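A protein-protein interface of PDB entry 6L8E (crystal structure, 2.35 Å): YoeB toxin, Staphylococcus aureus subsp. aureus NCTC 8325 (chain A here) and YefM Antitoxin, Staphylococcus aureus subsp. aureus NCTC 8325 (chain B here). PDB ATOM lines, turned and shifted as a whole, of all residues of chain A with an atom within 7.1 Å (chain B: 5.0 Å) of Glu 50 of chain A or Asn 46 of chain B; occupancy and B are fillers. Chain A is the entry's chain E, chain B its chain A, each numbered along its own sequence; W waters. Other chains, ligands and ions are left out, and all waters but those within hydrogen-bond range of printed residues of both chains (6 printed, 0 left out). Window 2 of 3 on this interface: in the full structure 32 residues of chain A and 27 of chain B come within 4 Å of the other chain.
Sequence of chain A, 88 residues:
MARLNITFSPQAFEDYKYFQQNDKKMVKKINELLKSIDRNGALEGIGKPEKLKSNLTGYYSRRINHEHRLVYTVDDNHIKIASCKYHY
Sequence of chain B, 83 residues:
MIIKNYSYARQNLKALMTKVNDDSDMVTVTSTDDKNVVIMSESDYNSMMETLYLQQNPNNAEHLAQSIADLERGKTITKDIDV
The side-chain hydroxyl (OG) of Ser 47 of chain B is in hydrogen-bond range of the backbone carbonyl oxygen (O) of Lys 51 of chain A, 3.3 Å away. The side-chain amino group (NZ) of Lys 53 of chain A lies within hydrogen-bond range of the side-chain hydroxyl (OG) of Ser 47 of chain B (3.3 Å). The side-chain carboxylate (OE2) of Glu 50 of chain B sits at hydrogen-bond distance from the side-chain hydroxyl (OG) of Ser 61 of chain A, at 2.8 Å.
OE2 of Glu 50 of chain A is in salt-bridge range of NZ of Lys 48 of chain A, at 3.0 Å. The backbone carbonyl oxygen (O) of Glu 42 of chain B sits close to the side-chain amide nitrogen (ND2) of Asn 46 of chain B. N of Glu 50 of chain A sits at hydrogen-bond distance from O of Ser 61 of chain A, at 3.0 Å.
Of chain B, only Asn 46, Ser 47 and Glu 50 come within 4 Å of Glu 50 of chain A. Of chain A, only Glu 50 (3.8 Å) comes within 4 Å of Asn 46 of chain B. Printed residues of chain A within 4 Å of Met 48 of chain B: Lys 53 (3.9 Å). Of the printed residues of chain B, Lys 51 of chain A touches Ser 47 (3.3 Å). Of the printed residues of chain B, Lys 53 of chain A touches Ser 47 and Met 48. Printed residues of chain A within 4 Å of Ser 47 of chain B: Glu 50, Lys 51 and Lys 53. Of the printed residues of chain B, Ser 61 of chain A touches Glu 50 (2.8 Å). Tyr 59 of chain A touches none of the printed residues of chain B. The nearest printed residue of chain A that does not touch Glu 50 of chain B is Leu 52 of chain A (4.1 Å).
Of the 9 printed residues of chain B, 4 touch a printed residue of chain A. Along chain A the printed residues that touch a printed residue of chain B span positions 50 to 61. Among the printed residues, 7 pairs touch across the chains. Among the printed residues, no Asp or Glu carboxylate lies within 4 Å of a Lys or Arg side-chain nitrogen of the other chain.
Among the printed residues, pairs that only touch across the chains: Glu 50 of chain A with Ser 47 of chain B (3.5 Å), Glu 50 of chain A with Asn 46 of chain B (3.8 Å), Glu 50 of chain A with Glu 50 of chain B (3.8 Å) and Lys 53 of chain A with Met 48 of chain B (3.9 Å).
Water W6 lies within hydrogen-bond range of NZ of Lys 53 of chain A, O of Lys 51 of chain A and OG of Ser 47 of chain B. Water W3 lies within hydrogen-bond range of the side-chain carboxylate (OE1) of Glu 50 of chain B, the guanidinium group (NE) of Arg 63 of chain A and the side-chain amino group (NZ) of Lys 48 of chain A. Water W5 bridges NZ of Lys 48 of chain A and O of Asn 46 of chain B. Water W2 lies within hydrogen-bond range of OE1 of Glu 50 of chain A (2.7 Å) and O of Ser 43 of chain B (2.9 Å). Water W4 bridges the side-chain carboxylate of Glu 50 of chain B (2.8 Å) and the guanidinium group of Arg 63 of chain A (3.1 Å). Water W1 lies within hydrogen-bond range of the side-chain hydroxyl (OG) of Ser 47 of chain B (2.8 Å), the backbone NH (N) of Lys 51 of chain A (2.9 Å) and the side-chain carboxylate (OE1) of Glu 50 of chain A (2.9 Å).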
ATOM      1  N   ALA A  42       8.855  35.294 -12.693  1.00  0.00           N
ATOM      2  CA  ALA A  42       8.066  34.113 -13.028  1.00  0.00           C
ATOM      3  C   ALA A  42       8.844  32.823 -12.797  1.00  0.00           C
ATOM      4  O   ALA A  42       8.271  31.812 -12.374  1.00  0.00           O
ATOM      5  CB  ALA A  42       7.596  34.200 -14.477  1.00  0.00           C
ATOM      6  N   LEU A  43      10.146  32.833 -13.070  1.00  0.00           N
ATOM      7  CA  LEU A  43      10.920  31.601 -13.158  1.00  0.00           C
ATOM      8  C   LEU A  43      11.847  31.346 -11.977  1.00  0.00           C
ATOM      9  O   LEU A  43      12.589  30.362 -12.008  1.00  0.00           O
ATOM     10  CB  LEU A  43      11.741  31.593 -14.451  1.00  0.00           C
ATOM     11  CG  LEU A  43      11.012  31.068 -15.687  1.00  0.00           C
ATOM     12  CD1 LEU A  43      11.953  30.970 -16.877  1.00  0.00           C
ATOM     13  CD2 LEU A  43      10.392  29.718 -15.381  1.00  0.00           C
ATOM     14  N   GLY A  47       8.720  26.504  -5.146  1.00  0.00           N
ATOM     15  CA  GLY A  47       7.605  25.903  -5.846  1.00  0.00           C
ATOM     16  C   GLY A  47       7.939  25.168  -7.125  1.00  0.00           C
ATOM     17  O   GLY A  47       7.015  24.686  -7.792  1.00  0.00           O
ATOM     18  N   LYS A  48       9.222  25.068  -7.489  1.00  0.00           N
ATOM     19  CA  LYS A  48       9.659  24.395  -8.709  1.00  0.00           C
ATOM     20  C   LYS A  48       8.997  25.035  -9.925  1.00  0.00           C
ATOM     21  O   LYS A  48       8.138  24.411 -10.562  1.00  0.00           O
ATOM     22  CB  LYS A  48       9.336  22.901  -8.629  1.00  0.00           C
ATOM     23  CG  LYS A  48       9.969  22.033  -9.703  1.00  0.00           C
ATOM     24  CD  LYS A  48       9.630  20.573  -9.455  1.00  0.00           C
ATOM     25  CE  LYS A  48       9.899  19.697 -10.669  1.00  0.00           C
ATOM     26  NZ  LYS A  48       8.835  19.851 -11.705  1.00  0.00           N
ATOM     27  N   PRO A  49       9.345  26.275 -10.269  1.00  0.00           N
ATOM     28  CA  PRO A  49       8.691  26.928 -11.411  1.00  0.00           C
ATOM     29  C   PRO A  49       9.014  26.201 -12.707  1.00  0.00           C
ATOM     30  O   PRO A  49      10.173  25.899 -12.997  1.00  0.00           O
ATOM     31  CB  PRO A  49       9.279  28.346 -11.402  1.00  0.00           C
ATOM     32  CG  PRO A  49       9.891  28.514 -10.043  1.00  0.00           C
ATOM     33  CD  PRO A  49      10.351  27.148  -9.644  1.00  0.00           C
ATOM     34  N   GLU A  50       7.976  25.913 -13.484  1.00  0.00           N
ATOM     35  CA  GLU A  50       8.132  25.362 -14.819  1.00  0.00           C
ATOM     36  C   GLU A  50       7.457  26.274 -15.832  1.00  0.00           C
ATOM     37  O   GLU A  50       6.437  26.908 -15.544  1.00  0.00           O
ATOM     38  CB  GLU A  50       7.544  23.950 -14.920  1.00  0.00           C
ATOM     39  CG  GLU A  50       8.157  22.949 -13.950  1.00  0.00           C
ATOM     40  CD  GLU A  50       9.540  22.483 -14.372  1.00  0.00           C
ATOM     41  OE1 GLU A  50       9.954  22.788 -15.512  1.00  0.00           O
ATOM     42  OE2 GLU A  50      10.214  21.810 -13.565  1.00  0.00           O
ATOM     43  N   LYS A  51       8.046  26.334 -17.024  1.00  0.00           N
ATOM     44  CA  LYS A  51       7.504  27.092 -18.143  1.00  0.00           C
ATOM     45  C   LYS A  51       6.629  26.164 -18.976  1.00  0.00           C
ATOM     46  O   LYS A  51       7.112  25.155 -19.499  1.00  0.00           O
ATOM     47  CB  LYS A  51       8.647  27.668 -18.977  1.00  0.00           C
ATOM     48  CG  LYS A  51       8.240  28.392 -20.237  1.00  0.00           C
ATOM     49  CD  LYS A  51       9.469  28.995 -20.903  1.00  0.00           C
ATOM     50  CE  LYS A  51       9.143  29.572 -22.270  1.00  0.00           C
ATOM     51  NZ  LYS A  51       7.969  30.485 -22.203  1.00  0.00           N
ATOM     52  N   LEU A  52       5.352  26.503 -19.101  1.00  0.00           N
ATOM     53  CA  LEU A  52       4.394  25.583 -19.690  1.00  0.00           C
ATOM     54  C   LEU A  52       4.453  25.618 -21.217  1.00  0.00           C
ATOM     55  O   LEU A  52       4.856  26.609 -21.835  1.00  0.00           O
ATOM     56  CB  LEU A  52       2.983  25.901 -19.194  1.00  0.00           C
ATOM     57  CG  LEU A  52       2.797  25.838 -17.674  1.00  0.00           C
ATOM     58  CD1 LEU A  52       1.327  25.964 -17.295  1.00  0.00           C
ATOM     59  CD2 LEU A  52       3.384  24.551 -17.117  1.00  0.00           C
ATOM     60  N   LYS A  53       4.028  24.515 -21.823  1.00  0.00           N
ATOM     61  CA  LYS A  53       4.117  24.304 -23.259  1.00  0.00           C
ATOM     62  C   LYS A  53       2.719  24.200 -23.868  1.00  0.00           C
ATOM     63  O   LYS A  53       1.701  24.298 -23.172  1.00  0.00           O
ATOM     64  CB  LYS A  53       4.929  23.040 -23.563  1.00  0.00           C
ATOM     65  CG  LYS A  53       6.323  23.018 -22.957  1.00  0.00           C
ATOM     66  CD  LYS A  53       7.002  21.682 -23.216  1.00  0.00           C
ATOM     67  CE  LYS A  53       8.305  21.568 -22.442  1.00  0.00           C
ATOM     68  NZ  LYS A  53       9.242  22.671 -22.797  1.00  0.00           N
ATOM     69  N   TYR A  59       2.358  30.793 -19.934  1.00  0.00           N
ATOM     70  CA  TYR A  59       2.018  30.620 -18.533  1.00  0.00           C
ATOM     71  C   TYR A  59       3.038  29.732 -17.840  1.00  0.00           C
ATOM     72  O   TYR A  59       3.812  29.009 -18.472  1.00  0.00           O
ATOM     73  CB  TYR A  59       0.609  30.039 -18.379  1.00  0.00           C
ATOM     74  CG  TYR A  59      -0.453  31.099 -18.521  1.00  0.00           C
ATOM     75  CD1 TYR A  59      -0.797  31.593 -19.771  1.00  0.00           C
ATOM     76  CD2 TYR A  59      -1.089  31.633 -17.405  1.00  0.00           C
ATOM     77  CE1 TYR A  59      -1.750  32.573 -19.917  1.00  0.00           C
ATOM     78  CE2 TYR A  59      -2.050  32.617 -17.541  1.00  0.00           C
ATOM     79  CZ  TYR A  59      -2.375  33.081 -18.806  1.00  0.00           C
ATOM     80  OH  TYR A  59      -3.326  34.059 -18.974  1.00  0.00           O
ATOM     81  N   TYR A  60       3.033  29.814 -16.517  1.00  0.00           N
ATOM     82  CA  TYR A  60       3.973  29.091 -15.687  1.00  0.00           C
ATOM     83  C   TYR A  60       3.201  28.370 -14.595  1.00  0.00           C
ATOM     84  O   TYR A  60       2.044  28.690 -14.314  1.00  0.00           O
ATOM     85  CB  TYR A  60       5.015  30.041 -15.077  1.00  0.00           C
ATOM     86  CG  TYR A  60       5.693  30.931 -16.097  1.00  0.00           C
ATOM     87  CD1 TYR A  60       5.064  32.080 -16.579  1.00  0.00           C
ATOM     88  CD2 TYR A  60       6.965  30.626 -16.573  1.00  0.00           C
ATOM     89  CE1 TYR A  60       5.681  32.894 -17.510  1.00  0.00           C
ATOM     90  CE2 TYR A  60       7.591  31.433 -17.503  1.00  0.00           C
ATOM     91  CZ  TYR A  60       6.947  32.563 -17.967  1.00  0.00           C
ATOM     92  OH  TYR A  60       7.588  33.354 -18.891  1.00  0.00           O
ATOM     93  N   SER A  61       3.850  27.385 -13.986  1.00  0.00           N
ATOM     94  CA  SER A  61       3.248  26.635 -12.898  1.00  0.00           C
ATOM     95  C   SER A  61       4.243  26.510 -11.756  1.00  0.00           C
ATOM     96  O   SER A  61       5.443  26.334 -11.975  1.00  0.00           O
ATOM     97  CB  SER A  61       2.780  25.247 -13.354  1.00  0.00           C
ATOM     98  OG  SER A  61       3.843  24.317 -13.321  1.00  0.00           O
ATOM     99  N   ARG A  62       3.733  26.649 -10.539  1.00  0.00           N
ATOM    100  CA  ARG A  62       4.455  26.286  -9.337  1.00  0.00           C
ATOM    101  C   ARG A  62       3.610  25.298  -8.551  1.00  0.00           C
ATOM    102  O   ARG A  62       2.385  25.246  -8.694  1.00  0.00           O
ATOM    103  CB  ARG A  62       4.792  27.513  -8.483  1.00  0.00           C
ATOM    104  CG  ARG A  62       5.775  28.443  -9.160  1.00  0.00           C
ATOM    105  CD  ARG A  62       6.277  29.522  -8.228  1.00  0.00           C
ATOM    106  NE  ARG A  62       7.019  30.535  -8.969  1.00  0.00           N
ATOM    107  CZ  ARG A  62       7.970  31.299  -8.445  1.00  0.00           C
ATOM    108  NH1 ARG A  62       8.306  31.159  -7.169  1.00  0.00           N
ATOM    109  NH2 ARG A  62       8.591  32.199  -9.199  1.00  0.00           N
ATOM    110  N   ARG A  63       4.279  24.503  -7.723  1.00  0.00           N
ATOM    111  CA  ARG A  63       3.595  23.488  -6.938  1.00  0.00           C
ATOM    112  C   ARG A  63       3.025  24.109  -5.669  1.00  0.00           C
ATOM    113  O   ARG A  63       3.760  24.710  -4.877  1.00  0.00           O
ATOM    114  CB  ARG A  63       4.544  22.342  -6.604  1.00  0.00           C
ATOM    115  CG  ARG A  63       4.996  21.593  -7.838  1.00  0.00           C
ATOM    116  CD  ARG A  63       5.615  20.255  -7.495  1.00  0.00           C
ATOM    117  NE  ARG A  63       5.863  19.472  -8.698  1.00  0.00           N
ATOM    118  CZ  ARG A  63       6.369  18.244  -8.692  1.00  0.00           C
ATOM    119  NH1 ARG A  63       6.677  17.666  -7.539  1.00  0.00           N
ATOM    120  NH2 ARG A  63       6.563  17.600  -9.836  1.00  0.00           N
ATOM    121  N   TYR A  72      -0.022  30.453 -13.622  1.00  0.00           N
ATOM    122  CA  TYR A  72      -0.017  31.907 -13.583  1.00  0.00           C
ATOM    123  C   TYR A  72       0.798  32.458 -14.744  1.00  0.00           C
ATOM    124  O   TYR A  72       1.511  31.729 -15.439  1.00  0.00           O
ATOM    125  CB  TYR A  72       0.553  32.412 -12.249  1.00  0.00           C
ATOM    126  CG  TYR A  72       2.006  32.036 -12.057  1.00  0.00           C
ATOM    127  CD1 TYR A  72       2.365  30.804 -11.517  1.00  0.00           C
ATOM    128  CD2 TYR A  72       3.019  32.910 -12.427  1.00  0.00           C
ATOM    129  CE1 TYR A  72       3.691  30.458 -11.350  1.00  0.00           C
ATOM    130  CE2 TYR A  72       4.346  32.574 -12.262  1.00  0.00           C
ATOM    131  CZ  TYR A  72       4.676  31.345 -11.721  1.00  0.00           C
ATOM    132  OH  TYR A  72       5.994  30.991 -11.549  1.00  0.00           O
ATOM    133  N   GLU B  42      17.405  16.167 -18.247  1.00  0.00           N
ATOM    134  CA  GLU B  42      16.507  16.134 -17.098  1.00  0.00           C
ATOM    135  C   GLU B  42      15.643  17.390 -17.043  1.00  0.00           C
ATOM    136  O   GLU B  42      14.459  17.322 -16.697  1.00  0.00           O
ATOM    137  CB  GLU B  42      17.310  15.963 -15.810  1.00  0.00           C
ATOM    138  CG  GLU B  42      16.559  15.232 -14.710  1.00  0.00           C
ATOM    139  CD  GLU B  42      17.401  15.024 -13.467  1.00  0.00           C
ATOM    140  OE1 GLU B  42      18.623  15.275 -13.532  1.00  0.00           O
ATOM    141  OE2 GLU B  42      16.845  14.618 -12.426  1.00  0.00           O
ATOM    142  N   SER B  43      16.216  18.543 -17.408  1.00  0.00           N
ATOM    143  CA  SER B  43      15.465  19.795 -17.409  1.00  0.00           C
ATOM    144  C   SER B  43      14.303  19.738 -18.391  1.00  0.00           C
ATOM    145  O   SER B  43      13.181  20.150 -18.069  1.00  0.00           O
ATOM    146  CB  SER B  43      16.394  20.959 -17.746  1.00  0.00           C
ATOM    147  OG  SER B  43      15.769  22.208 -17.503  1.00  0.00           O
ATOM    148  N   ASP B  44      14.550  19.222 -19.595  1.00  0.00           N
ATOM    149  CA  ASP B  44      13.480  19.103 -20.579  1.00  0.00           C
ATOM    150  C   ASP B  44      12.439  18.085 -20.141  1.00  0.00           C
ATOM    151  O   ASP B  44      11.241  18.271 -20.389  1.00  0.00           O
ATOM    152  CB  ASP B  44      14.056  18.727 -21.942  1.00  0.00           C
ATOM    153  CG  ASP B  44      14.689  19.904 -22.647  1.00  0.00           C
ATOM    154  OD1 ASP B  44      14.919  20.935 -21.981  1.00  0.00           O
ATOM    155  OD2 ASP B  44      14.945  19.806 -23.864  1.00  0.00           O
ATOM    156  N   TYR B  45      12.876  17.001 -19.498  1.00  0.00           N
ATOM    157  CA  TYR B  45      11.936  15.992 -19.025  1.00  0.00           C
ATOM    158  C   TYR B  45      11.010  16.569 -17.963  1.00  0.00           C
ATOM    159  O   TYR B  45       9.790  16.379 -18.018  1.00  0.00           O
ATOM    160  CB  TYR B  45      12.692  14.786 -18.471  1.00  0.00           C
ATOM    161  CG  TYR B  45      11.805  13.809 -17.739  1.00  0.00           C
ATOM    162  CD1 TYR B  45      10.990  12.933 -18.439  1.00  0.00           C
ATOM    163  CD2 TYR B  45      11.780  13.761 -16.350  1.00  0.00           C
ATOM    164  CE1 TYR B  45      10.180  12.037 -17.782  1.00  0.00           C
ATOM    165  CE2 TYR B  45      10.971  12.864 -15.684  1.00  0.00           C
ATOM    166  CZ  TYR B  45      10.172  12.005 -16.404  1.00  0.00           C
ATOM    167  OH  TYR B  45       9.360  11.108 -15.748  1.00  0.00           O
ATOM    168  N   ASN B  46      11.583  17.276 -16.984  1.00  0.00           N
ATOM    169  CA  ASN B  46      10.774  17.917 -15.953  1.00  0.00           C
ATOM    170  C   ASN B  46       9.771  18.885 -16.564  1.00  0.00           C
ATOM    171  O   ASN B  46       8.597  18.904 -16.179  1.00  0.00           O
ATOM    172  CB  ASN B  46      11.672  18.644 -14.950  1.00  0.00           C
ATOM    173  CG  ASN B  46      12.464  17.696 -14.080  1.00  0.00           C
ATOM    174  OD1 ASN B  46      12.080  16.542 -13.886  1.00  0.00           O
ATOM    175  ND2 ASN B  46      13.581  18.176 -13.547  1.00  0.00           N
ATOM    176  N   SER B  47      10.219  19.703 -17.521  1.00  0.00           N
ATOM    177  CA  SER B  47       9.321  20.659 -18.161  1.00  0.00           C
ATOM    178  C   SER B  47       8.203  19.937 -18.904  1.00  0.00           C
ATOM    179  O   SER B  47       7.027  20.310 -18.804  1.00  0.00           O
ATOM    180  CB  SER B  47      10.109  21.559 -19.112  1.00  0.00           C
ATOM    181  OG  SER B  47       9.324  22.662 -19.517  1.00  0.00           O
ATOM    182  N   MET B  48       8.554  18.879 -19.635  1.00  0.00           N
ATOM    183  CA  MET B  48       7.567  18.133 -20.407  1.00  0.00           C
ATOM    184  C   MET B  48       6.532  17.482 -19.499  1.00  0.00           C
ATOM    185  O   MET B  48       5.327  17.543 -19.768  1.00  0.00           O
ATOM    186  CB  MET B  48       8.271  17.074 -21.255  1.00  0.00           C
ATOM    187  CG  MET B  48       7.337  16.240 -22.119  1.00  0.00           C
ATOM    188  SD  MET B  48       8.179  14.867 -22.928  1.00  0.00           S
ATOM    189  CE  MET B  48       6.941  14.359 -24.120  1.00  0.00           C
ATOM    190  N   MET B  49       6.986  16.838 -18.421  1.00  0.00           N
ATOM    191  CA  MET B  49       6.059  16.127 -17.547  1.00  0.00           C
ATOM    192  C   MET B  49       5.105  17.077 -16.832  1.00  0.00           C
ATOM    193  O   MET B  49       3.961  16.702 -16.556  1.00  0.00           O
ATOM    194  CB  MET B  49       6.829  15.291 -16.525  1.00  0.00           C
ATOM    195  CG  MET B  49       7.605  14.149 -17.146  1.00  0.00           C
ATOM    196  SD  MET B  49       6.588  13.066 -18.169  1.00  0.00           S
ATOM    197  CE  MET B  49       5.588  12.246 -16.927  1.00  0.00           C
ATOM    198  N   GLU B  50       5.548  18.302 -16.527  1.00  0.00           N
ATOM    199  CA  GLU B  50       4.685  19.229 -15.799  1.00  0.00           C
ATOM    200  C   GLU B  50       3.523  19.699 -16.666  1.00  0.00           C
ATOM    201  O   GLU B  50       2.374  19.743 -16.206  1.00  0.00           O
ATOM    202  CB  GLU B  50       5.491  20.418 -15.276  1.00  0.00           C
ATOM    203  CG  GLU B  50       4.638  21.528 -14.650  1.00  0.00           C
ATOM    204  CD  GLU B  50       3.788  21.057 -13.472  1.00  0.00           C
ATOM    205  OE1 GLU B  50       4.121  20.011 -12.868  1.00  0.00           O
ATOM    206  OE2 GLU B  50       2.780  21.739 -13.161  1.00  0.00           O
HETATM  207  O   HOH W   1      10.225  24.651 -17.765  1.00  0.00           O
HETATM  208  O   HOH W   2      12.571  22.160 -16.060  1.00  0.00           O
HETATM  209  O   HOH W   3       5.909  20.625 -11.204  1.00  0.00           O
HETATM  210  O   HOH W   4       5.323  17.545 -12.650  1.00  0.00           O
HETATM  211  O   HOH W   5       7.819  18.132 -13.527  1.00  0.00           O
HETATM  212  O   HOH W   6       9.001  24.873 -21.674  1.00  0.00           O
